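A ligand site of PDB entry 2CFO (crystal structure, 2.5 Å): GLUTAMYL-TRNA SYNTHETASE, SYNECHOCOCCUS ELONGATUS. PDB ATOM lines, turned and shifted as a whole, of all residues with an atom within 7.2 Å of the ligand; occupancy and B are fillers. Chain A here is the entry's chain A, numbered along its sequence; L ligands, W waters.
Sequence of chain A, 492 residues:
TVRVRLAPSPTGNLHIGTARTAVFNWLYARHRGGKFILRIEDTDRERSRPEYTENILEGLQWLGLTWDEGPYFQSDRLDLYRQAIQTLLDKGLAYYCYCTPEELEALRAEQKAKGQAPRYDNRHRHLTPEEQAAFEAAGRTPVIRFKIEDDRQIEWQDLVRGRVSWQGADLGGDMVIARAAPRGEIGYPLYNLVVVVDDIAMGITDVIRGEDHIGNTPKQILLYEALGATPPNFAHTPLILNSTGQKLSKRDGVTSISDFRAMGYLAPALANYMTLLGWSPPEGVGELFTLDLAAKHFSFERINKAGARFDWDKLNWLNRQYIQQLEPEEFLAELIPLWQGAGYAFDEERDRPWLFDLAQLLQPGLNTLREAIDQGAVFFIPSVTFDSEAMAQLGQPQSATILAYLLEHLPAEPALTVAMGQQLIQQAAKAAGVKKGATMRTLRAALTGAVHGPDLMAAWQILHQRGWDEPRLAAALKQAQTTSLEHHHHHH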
ATOM      1  N   ARG A   5     -16.268  32.075 -27.882  1.00  0.00           N
ATOM      2  CA  ARG A   5     -15.658  32.033 -26.562  1.00  0.00           C
ATOM      3  C   ARG A   5     -16.076  30.838 -25.716  1.00  0.00           C
ATOM      4  O   ARG A   5     -17.185  30.353 -25.840  1.00  0.00           O
ATOM      5  CB  ARG A   5     -15.963  33.359 -25.803  1.00  0.00           C
ATOM      6  CG  ARG A   5     -17.349  33.538 -25.099  1.00  0.00           C
ATOM      7  CD  ARG A   5     -18.571  33.435 -26.023  1.00  0.00           C
ATOM      8  NE  ARG A   5     -19.796  33.796 -25.308  1.00  0.00           N
ATOM      9  CZ  ARG A   5     -20.591  32.926 -24.664  1.00  0.00           C
ATOM     10  NH1 ARG A   5     -20.332  31.626 -24.638  1.00  0.00           N
ATOM     11  NH2 ARG A   5     -21.662  33.373 -24.033  1.00  0.00           N
ATOM     12  N   LEU A   6     -15.176  30.362 -24.870  1.00  0.00           N
ATOM     13  CA  LEU A   6     -15.572  29.418 -23.864  1.00  0.00           C
ATOM     14  C   LEU A   6     -15.715  30.212 -22.576  1.00  0.00           C
ATOM     15  O   LEU A   6     -14.871  31.085 -22.287  1.00  0.00           O
ATOM     16  CB  LEU A   6     -14.560  28.285 -23.723  1.00  0.00           C
ATOM     17  CG  LEU A   6     -15.079  27.100 -22.890  1.00  0.00           C
ATOM     18  CD1 LEU A   6     -16.060  26.182 -23.653  1.00  0.00           C
ATOM     19  CD2 LEU A   6     -13.928  26.298 -22.381  1.00  0.00           C
ATOM     20  N   ALA A   7     -16.797  29.958 -21.840  1.00  0.00           N
ATOM     21  CA  ALA A   7     -17.018  30.699 -20.586  1.00  0.00           C
ATOM     22  C   ALA A   7     -17.267  29.754 -19.389  1.00  0.00           C
ATOM     23  O   ALA A   7     -18.343  29.776 -18.757  1.00  0.00           O
ATOM     24  CB  ALA A   7     -18.136  31.739 -20.743  1.00  0.00           C
ATOM     25  N   PRO A   8     -16.225  28.966 -19.037  1.00  0.00           N
ATOM     26  CA  PRO A   8     -16.479  28.060 -17.936  1.00  0.00           C
ATOM     27  C   PRO A   8     -16.394  28.762 -16.595  1.00  0.00           C
ATOM     28  O   PRO A   8     -15.712  29.793 -16.471  1.00  0.00           O
ATOM     29  CB  PRO A   8     -15.369  27.006 -18.085  1.00  0.00           C
ATOM     30  CG  PRO A   8     -14.309  27.667 -18.804  1.00  0.00           C
ATOM     31  CD  PRO A   8     -14.842  28.864 -19.523  1.00  0.00           C
ATOM     32  N   SER A   9     -17.197  28.287 -15.658  1.00  0.00           N
ATOM     33  CA  SER A   9     -17.063  28.676 -14.273  1.00  0.00           C
ATOM     34  C   SER A   9     -16.128  27.658 -13.645  1.00  0.00           C
ATOM     35  O   SER A   9     -16.338  26.443 -13.825  1.00  0.00           O
ATOM     36  CB  SER A   9     -18.413  28.644 -13.581  1.00  0.00           C
ATOM     37  OG  SER A   9     -18.935  27.334 -13.619  1.00  0.00           O
ATOM     38  N   GLY A  17     -18.715  17.673 -21.123  1.00  0.00           N
ATOM     39  CA  GLY A  17     -19.717  18.563 -21.709  1.00  0.00           C
ATOM     40  C   GLY A  17     -19.128  19.896 -22.119  1.00  0.00           C
ATOM     41  O   GLY A  17     -19.317  20.359 -23.266  1.00  0.00           O
ATOM     42  N   THR A  18     -18.361  20.487 -21.200  1.00  0.00           N
ATOM     43  CA  THR A  18     -17.761  21.785 -21.418  1.00  0.00           C
ATOM     44  C   THR A  18     -16.719  21.689 -22.498  1.00  0.00           C
ATOM     45  O   THR A  18     -16.758  22.455 -23.445  1.00  0.00           O
ATOM     46  CB  THR A  18     -17.128  22.320 -20.147  1.00  0.00           C
ATOM     47  OG1 THR A  18     -18.113  22.317 -19.114  1.00  0.00           O
ATOM     48  CG2 THR A  18     -16.585  23.731 -20.354  1.00  0.00           C
ATOM     49  N   THR A  21     -18.239  21.522 -25.927  1.00  0.00           N
ATOM     50  CA  THR A  21     -18.589  22.848 -26.355  1.00  0.00           C
ATOM     51  C   THR A  21     -17.332  23.584 -26.842  1.00  0.00           C
ATOM     52  O   THR A  21     -17.362  24.206 -27.933  1.00  0.00           O
ATOM     53  CB  THR A  21     -19.303  23.576 -25.216  1.00  0.00           C
ATOM     54  OG1 THR A  21     -20.561  22.946 -25.008  1.00  0.00           O
ATOM     55  CG2 THR A  21     -19.524  25.062 -25.534  1.00  0.00           C
ATOM     56  N   ASN A  25     -16.524  25.166 -30.558  1.00  0.00           N
ATOM     57  CA  ASN A  25     -16.072  26.547 -30.690  1.00  0.00           C
ATOM     58  C   ASN A  25     -14.761  26.664 -31.464  1.00  0.00           C
ATOM     59  O   ASN A  25     -14.667  27.424 -32.391  1.00  0.00           O
ATOM     60  CB  ASN A  25     -15.953  27.213 -29.328  1.00  0.00           C
ATOM     61  CG  ASN A  25     -17.287  27.632 -28.770  1.00  0.00           C
ATOM     62  OD1 ASN A  25     -17.854  28.665 -29.160  1.00  0.00           O
ATOM     63  ND2 ASN A  25     -17.790  26.850 -27.828  1.00  0.00           N
ATOM     64  N   ARG A  39     -12.838  32.874 -21.414  1.00  0.00           N
ATOM     65  CA  ARG A  39     -13.274  33.764 -20.358  1.00  0.00           C
ATOM     66  C   ARG A  39     -13.517  32.894 -19.135  1.00  0.00           C
ATOM     67  O   ARG A  39     -14.189  31.872 -19.240  1.00  0.00           O
ATOM     68  CB  ARG A  39     -14.544  34.486 -20.808  1.00  0.00           C
ATOM     69  CG  ARG A  39     -15.013  35.600 -19.913  1.00  0.00           C
ATOM     70  CD  ARG A  39     -15.965  36.502 -20.619  1.00  0.00           C
ATOM     71  NE  ARG A  39     -17.282  35.893 -20.840  1.00  0.00           N
ATOM     72  CZ  ARG A  39     -18.075  36.103 -21.899  1.00  0.00           C
ATOM     73  NH1 ARG A  39     -17.690  36.913 -22.888  1.00  0.00           N
ATOM     74  NH2 ARG A  39     -19.238  35.493 -21.984  1.00  0.00           N
ATOM     75  N   GLU A  41     -15.222  32.587 -15.587  1.00  0.00           N
ATOM     76  CA  GLU A  41     -16.275  33.192 -14.808  1.00  0.00           C
ATOM     77  C   GLU A  41     -16.038  32.944 -13.333  1.00  0.00           C
ATOM     78  O   GLU A  41     -16.842  32.267 -12.662  1.00  0.00           O
ATOM     79  CB  GLU A  41     -17.645  32.685 -15.282  1.00  0.00           C
ATOM     80  CG  GLU A  41     -17.928  33.040 -16.739  1.00  0.00           C
ATOM     81  CD  GLU A  41     -19.380  32.804 -17.158  1.00  0.00           C
ATOM     82  OE1 GLU A  41     -19.919  31.692 -16.918  1.00  0.00           O
ATOM     83  OE2 GLU A  41     -19.950  33.742 -17.781  1.00  0.00           O
ATOM     84  N   TYR A 191     -25.573  35.903 -13.716  1.00  0.00           N
ATOM     85  CA  TYR A 191     -25.007  35.310 -14.955  1.00  0.00           C
ATOM     86  C   TYR A 191     -25.402  36.002 -16.260  1.00  0.00           C
ATOM     87  O   TYR A 191     -24.522  36.357 -17.057  1.00  0.00           O
ATOM     88  CB  TYR A 191     -25.269  33.765 -15.034  1.00  0.00           C
ATOM     89  CG  TYR A 191     -25.162  33.222 -16.462  1.00  0.00           C
ATOM     90  CD1 TYR A 191     -23.895  33.094 -17.120  1.00  0.00           C
ATOM     91  CD2 TYR A 191     -26.332  32.932 -17.203  1.00  0.00           C
ATOM     92  CE1 TYR A 191     -23.803  32.663 -18.476  1.00  0.00           C
ATOM     93  CE2 TYR A 191     -26.240  32.500 -18.559  1.00  0.00           C
ATOM     94  CZ  TYR A 191     -24.993  32.373 -19.183  1.00  0.00           C
ATOM     95  OH  TYR A 191     -24.931  31.964 -20.487  1.00  0.00           O
ATOM     96  N   VAL A 195     -22.711  37.806 -18.886  1.00  0.00           N
ATOM     97  CA  VAL A 195     -22.422  37.181 -20.147  1.00  0.00           C
ATOM     98  C   VAL A 195     -22.672  38.122 -21.370  1.00  0.00           C
ATOM     99  O   VAL A 195     -21.851  38.141 -22.292  1.00  0.00           O
ATOM    100  CB  VAL A 195     -23.166  35.846 -20.268  1.00  0.00           C
ATOM    101  CG1 VAL A 195     -24.647  36.094 -20.444  1.00  0.00           C
ATOM    102  CG2 VAL A 195     -22.644  35.031 -21.391  1.00  0.00           C
ATOM    103  N   ASP A 199     -19.958  39.547 -23.642  1.00  0.00           N
ATOM    104  CA  ASP A 199     -20.073  39.193 -25.051  1.00  0.00           C
ATOM    105  C   ASP A 199     -20.097  40.402 -25.947  1.00  0.00           C
ATOM    106  O   ASP A 199     -19.553  40.347 -27.053  1.00  0.00           O
ATOM    107  CB  ASP A 199     -21.277  38.297 -25.319  1.00  0.00           C
ATOM    108  CG  ASP A 199     -21.035  36.847 -24.849  1.00  0.00           C
ATOM    109  OD1 ASP A 199     -19.866  36.492 -24.496  1.00  0.00           O
ATOM    110  OD2 ASP A 199     -22.027  36.080 -24.831  1.00  0.00           O
ATOM    111  N   VAL A 207     -22.478  32.485 -30.300  1.00  0.00           N
ATOM    112  CA  VAL A 207     -22.444  31.850 -28.963  1.00  0.00           C
ATOM    113  C   VAL A 207     -22.842  30.392 -29.135  1.00  0.00           C
ATOM    114  O   VAL A 207     -23.889  30.092 -29.723  1.00  0.00           O
ATOM    115  CB  VAL A 207     -23.364  32.602 -27.957  1.00  0.00           C
ATOM    116  CG1 VAL A 207     -23.452  31.889 -26.598  1.00  0.00           C
ATOM    117  CG2 VAL A 207     -22.873  34.024 -27.776  1.00  0.00           C
ATOM    118  N   ILE A 208     -21.973  29.490 -28.686  1.00  0.00           N
ATOM    119  CA  ILE A 208     -22.284  28.039 -28.749  1.00  0.00           C
ATOM    120  C   ILE A 208     -22.631  27.556 -27.371  1.00  0.00           C
ATOM    121  O   ILE A 208     -21.874  27.713 -26.430  1.00  0.00           O
ATOM    122  CB  ILE A 208     -21.175  27.184 -29.423  1.00  0.00           C
ATOM    123  CG1 ILE A 208     -20.943  27.650 -30.857  1.00  0.00           C
ATOM    124  CG2 ILE A 208     -21.531  25.685 -29.431  1.00  0.00           C
ATOM    125  CD1 ILE A 208     -19.660  27.079 -31.443  1.00  0.00           C
ATOM    126  N   ARG A 209     -23.802  26.992 -27.264  1.00  0.00           N
ATOM    127  CA  ARG A 209     -24.345  26.632 -25.955  1.00  0.00           C
ATOM    128  C   ARG A 209     -25.046  25.307 -25.982  1.00  0.00           C
ATOM    129  O   ARG A 209     -25.492  24.860 -27.039  1.00  0.00           O
ATOM    130  CB  ARG A 209     -25.351  27.691 -25.524  1.00  0.00           C
ATOM    131  CG  ARG A 209     -24.745  28.908 -24.984  1.00  0.00           C
ATOM    132  CD  ARG A 209     -25.604  29.418 -23.893  1.00  0.00           C
ATOM    133  NE  ARG A 209     -26.657  30.272 -24.358  1.00  0.00           N
ATOM    134  CZ  ARG A 209     -26.652  31.583 -24.206  1.00  0.00           C
ATOM    135  NH1 ARG A 209     -25.641  32.161 -23.561  1.00  0.00           N
ATOM    136  NH2 ARG A 209     -27.664  32.330 -24.680  1.00  0.00           N
ATOM    137  N   GLY A 210     -25.133  24.668 -24.809  1.00  0.00           N
ATOM    138  CA  GLY A 210     -25.926  23.483 -24.613  1.00  0.00           C
ATOM    139  C   GLY A 210     -27.381  23.915 -24.636  1.00  0.00           C
ATOM    140  O   GLY A 210     -27.731  25.052 -24.192  1.00  0.00           O
ATOM    141  N   GLU A 211     -28.230  23.005 -25.148  1.00  0.00           N
ATOM    142  CA  GLU A 211     -29.666  23.248 -25.285  1.00  0.00           C
ATOM    143  C   GLU A 211     -30.355  23.310 -23.916  1.00  0.00           C
ATOM    144  O   GLU A 211     -31.495  23.783 -23.813  1.00  0.00           O
ATOM    145  CB  GLU A 211     -30.349  22.196 -26.232  1.00  0.00           C
ATOM    146  CG  GLU A 211     -30.798  20.853 -25.565  1.00  0.00           C
ATOM    147  CD  GLU A 211     -31.088  19.716 -26.570  1.00  0.00           C
ATOM    148  OE1 GLU A 211     -30.915  19.968 -27.781  1.00  0.00           O
ATOM    149  OE2 GLU A 211     -31.442  18.572 -26.152  1.00  0.00           O
ATOM    150  N   ASP A 212     -29.682  22.833 -22.879  1.00  0.00           N
ATOM    151  CA  ASP A 212     -30.255  22.934 -21.546  1.00  0.00           C
ATOM    152  C   ASP A 212     -30.302  24.385 -21.021  1.00  0.00           C
ATOM    153  O   ASP A 212     -31.048  24.670 -20.082  1.00  0.00           O
ATOM    154  CB  ASP A 212     -29.577  21.955 -20.559  1.00  0.00           C
ATOM    155  CG  ASP A 212     -28.106  22.267 -20.314  1.00  0.00           C
ATOM    156  OD1 ASP A 212     -27.388  22.815 -21.220  1.00  0.00           O
ATOM    157  OD2 ASP A 212     -27.658  21.918 -19.190  1.00  0.00           O
ATOM    158  N   HIS A 213     -29.556  25.300 -21.671  1.00  0.00           N
ATOM    159  CA  HIS A 213     -29.576  26.742 -21.315  1.00  0.00           C
ATOM    160  C   HIS A 213     -30.234  27.631 -22.382  1.00  0.00           C
ATOM    161  O   HIS A 213     -30.065  28.872 -22.377  1.00  0.00           O
ATOM    162  CB  HIS A 213     -28.164  27.256 -20.921  1.00  0.00           C
ATOM    163  CG  HIS A 213     -27.510  26.444 -19.856  1.00  0.00           C
ATOM    164  ND1 HIS A 213     -26.188  26.045 -19.923  1.00  0.00           N
ATOM    165  CD2 HIS A 213     -28.011  25.891 -18.718  1.00  0.00           C
ATOM    166  CE1 HIS A 213     -25.902  25.299 -18.866  1.00  0.00           C
ATOM    167  NE2 HIS A 213     -26.983  25.193 -18.120  1.00  0.00           N
ATOM    168  N   ASN A 216     -32.137  31.013 -21.458  1.00  0.00           N
ATOM    169  CA  ASN A 216     -31.384  32.223 -21.098  1.00  0.00           C
ATOM    170  C   ASN A 216     -31.235  33.062 -22.330  1.00  0.00           C
ATOM    171  O   ASN A 216     -31.035  34.281 -22.248  1.00  0.00           O
ATOM    172  CB  ASN A 216     -29.983  31.875 -20.574  1.00  0.00           C
ATOM    173  CG  ASN A 216     -29.987  31.237 -19.144  1.00  0.00           C
ATOM    174  OD1 ASN A 216     -30.951  31.411 -18.366  1.00  0.00           O
ATOM    175  ND2 ASN A 216     -28.896  30.538 -18.787  1.00  0.00           N
ATOM    176  N   GLN A 220     -31.145  37.063 -22.515  1.00  0.00           N
ATOM    177  CA  GLN A 220     -29.935  37.755 -22.879  1.00  0.00           C
ATOM    178  C   GLN A 220     -30.214  38.684 -24.061  1.00  0.00           C
ATOM    179  O   GLN A 220     -29.828  39.834 -24.031  1.00  0.00           O
ATOM    180  CB  GLN A 220     -28.868  36.741 -23.193  1.00  0.00           C
ATOM    181  CG  GLN A 220     -28.368  36.034 -21.942  1.00  0.00           C
ATOM    182  CD  GLN A 220     -27.390  34.931 -22.238  1.00  0.00           C
ATOM    183  OE1 GLN A 220     -26.847  34.845 -23.333  1.00  0.00           O
ATOM    184  NE2 GLN A 220     -27.137  34.083 -21.223  1.00  0.00           N
ATOM    185  N   LEU A 239     -27.156  17.929 -25.451  1.00  0.00           N
ATOM    186  CA  LEU A 239     -26.188  17.471 -24.473  1.00  0.00           C
ATOM    187  C   LEU A 239     -25.688  16.078 -24.815  1.00  0.00           C
ATOM    188  O   LEU A 239     -26.245  15.414 -25.714  1.00  0.00           O
ATOM    189  CB  LEU A 239     -26.777  17.456 -23.045  1.00  0.00           C
ATOM    190  CG  LEU A 239     -27.242  18.690 -22.252  1.00  0.00           C
ATOM    191  CD1 LEU A 239     -26.213  19.824 -22.205  1.00  0.00           C
ATOM    192  CD2 LEU A 239     -28.612  19.195 -22.782  1.00  0.00           C
HETATM  193  N1  LIG L   1     -21.876  27.429 -19.228  1.00  0.00           N
HETATM  194  C1  LIG L   1     -23.058  27.460 -20.130  1.00  0.00           C
HETATM  195  C2  LIG L   1     -22.859  26.661 -21.444  1.00  0.00           C
HETATM  196  O1  LIG L   1     -23.707  25.837 -21.840  1.00  0.00           O
HETATM  197  C3  LIG L   1     -23.455  28.894 -20.448  1.00  0.00           C
HETATM  198  C4  LIG L   1     -22.284  29.842 -20.664  1.00  0.00           C
HETATM  199  C5  LIG L   1     -22.339  30.535 -22.001  1.00  0.00           C
HETATM  200  O2  LIG L   1     -21.858  29.949 -22.988  1.00  0.00           O
HETATM  201  O3  LIG L   1     -22.821  31.676 -22.064  1.00  0.00           O
HETATM  202  O4  LIG L   1     -21.862  26.817 -22.159  1.00  0.00           O
HETATM  203  O   HOH W   1     -19.146  26.772 -19.649  1.00  0.00           O
HETATM  204  O   HOH W   2     -24.487  22.675 -21.685  1.00  0.00           O
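OH of Tyr 191 is in hydrogen-bond range of NH1 of Arg 209, at 3.2 Å. NE2 of Gln 220 is in hydrogen-bond range of OH of Tyr 191 (3.1 Å). The side-chain carboxylate (OD1) of Asp 199 is in salt-bridge range of the guanidinium group (NE) of Arg 5. NH1 of Arg 209 is in hydrogen-bond range of OE1 of Gln 220, at 3.0 Å.
Residues that only touch the ligand: Val 195. Of the 24 residues printed, 6 come within 4 Å of the ligand.
OH of Tyr 191 lies within hydrogen-bond range of O3 of the ligand (2.6 Å). The guanidinium group (NH1) of Arg 5 is in salt-bridge range of an oxygen (O2) of the ligand, at 2.8 Å. An oxygen (O1) of the ligand sits at hydrogen-bond distance from a ring nitrogen (ND1) of His 213 (3.1 Å). The guanidinium group (NH1) of Arg 209 lies within salt-bridge range of an oxygen (O3) of the ligand (3.2 Å). An oxygen (O1) of the ligand lies within hydrogen-bond range of the backbone NH of Gly 210, 3.5 Å away.
Water W1 lies within hydrogen-bond range of N1 of the ligand and O of Ala 7. Water W2 lies within hydrogen-bond range of the side-chain carboxylate (OD1) of Asp 212 and an oxygen (O1) of the ligand.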
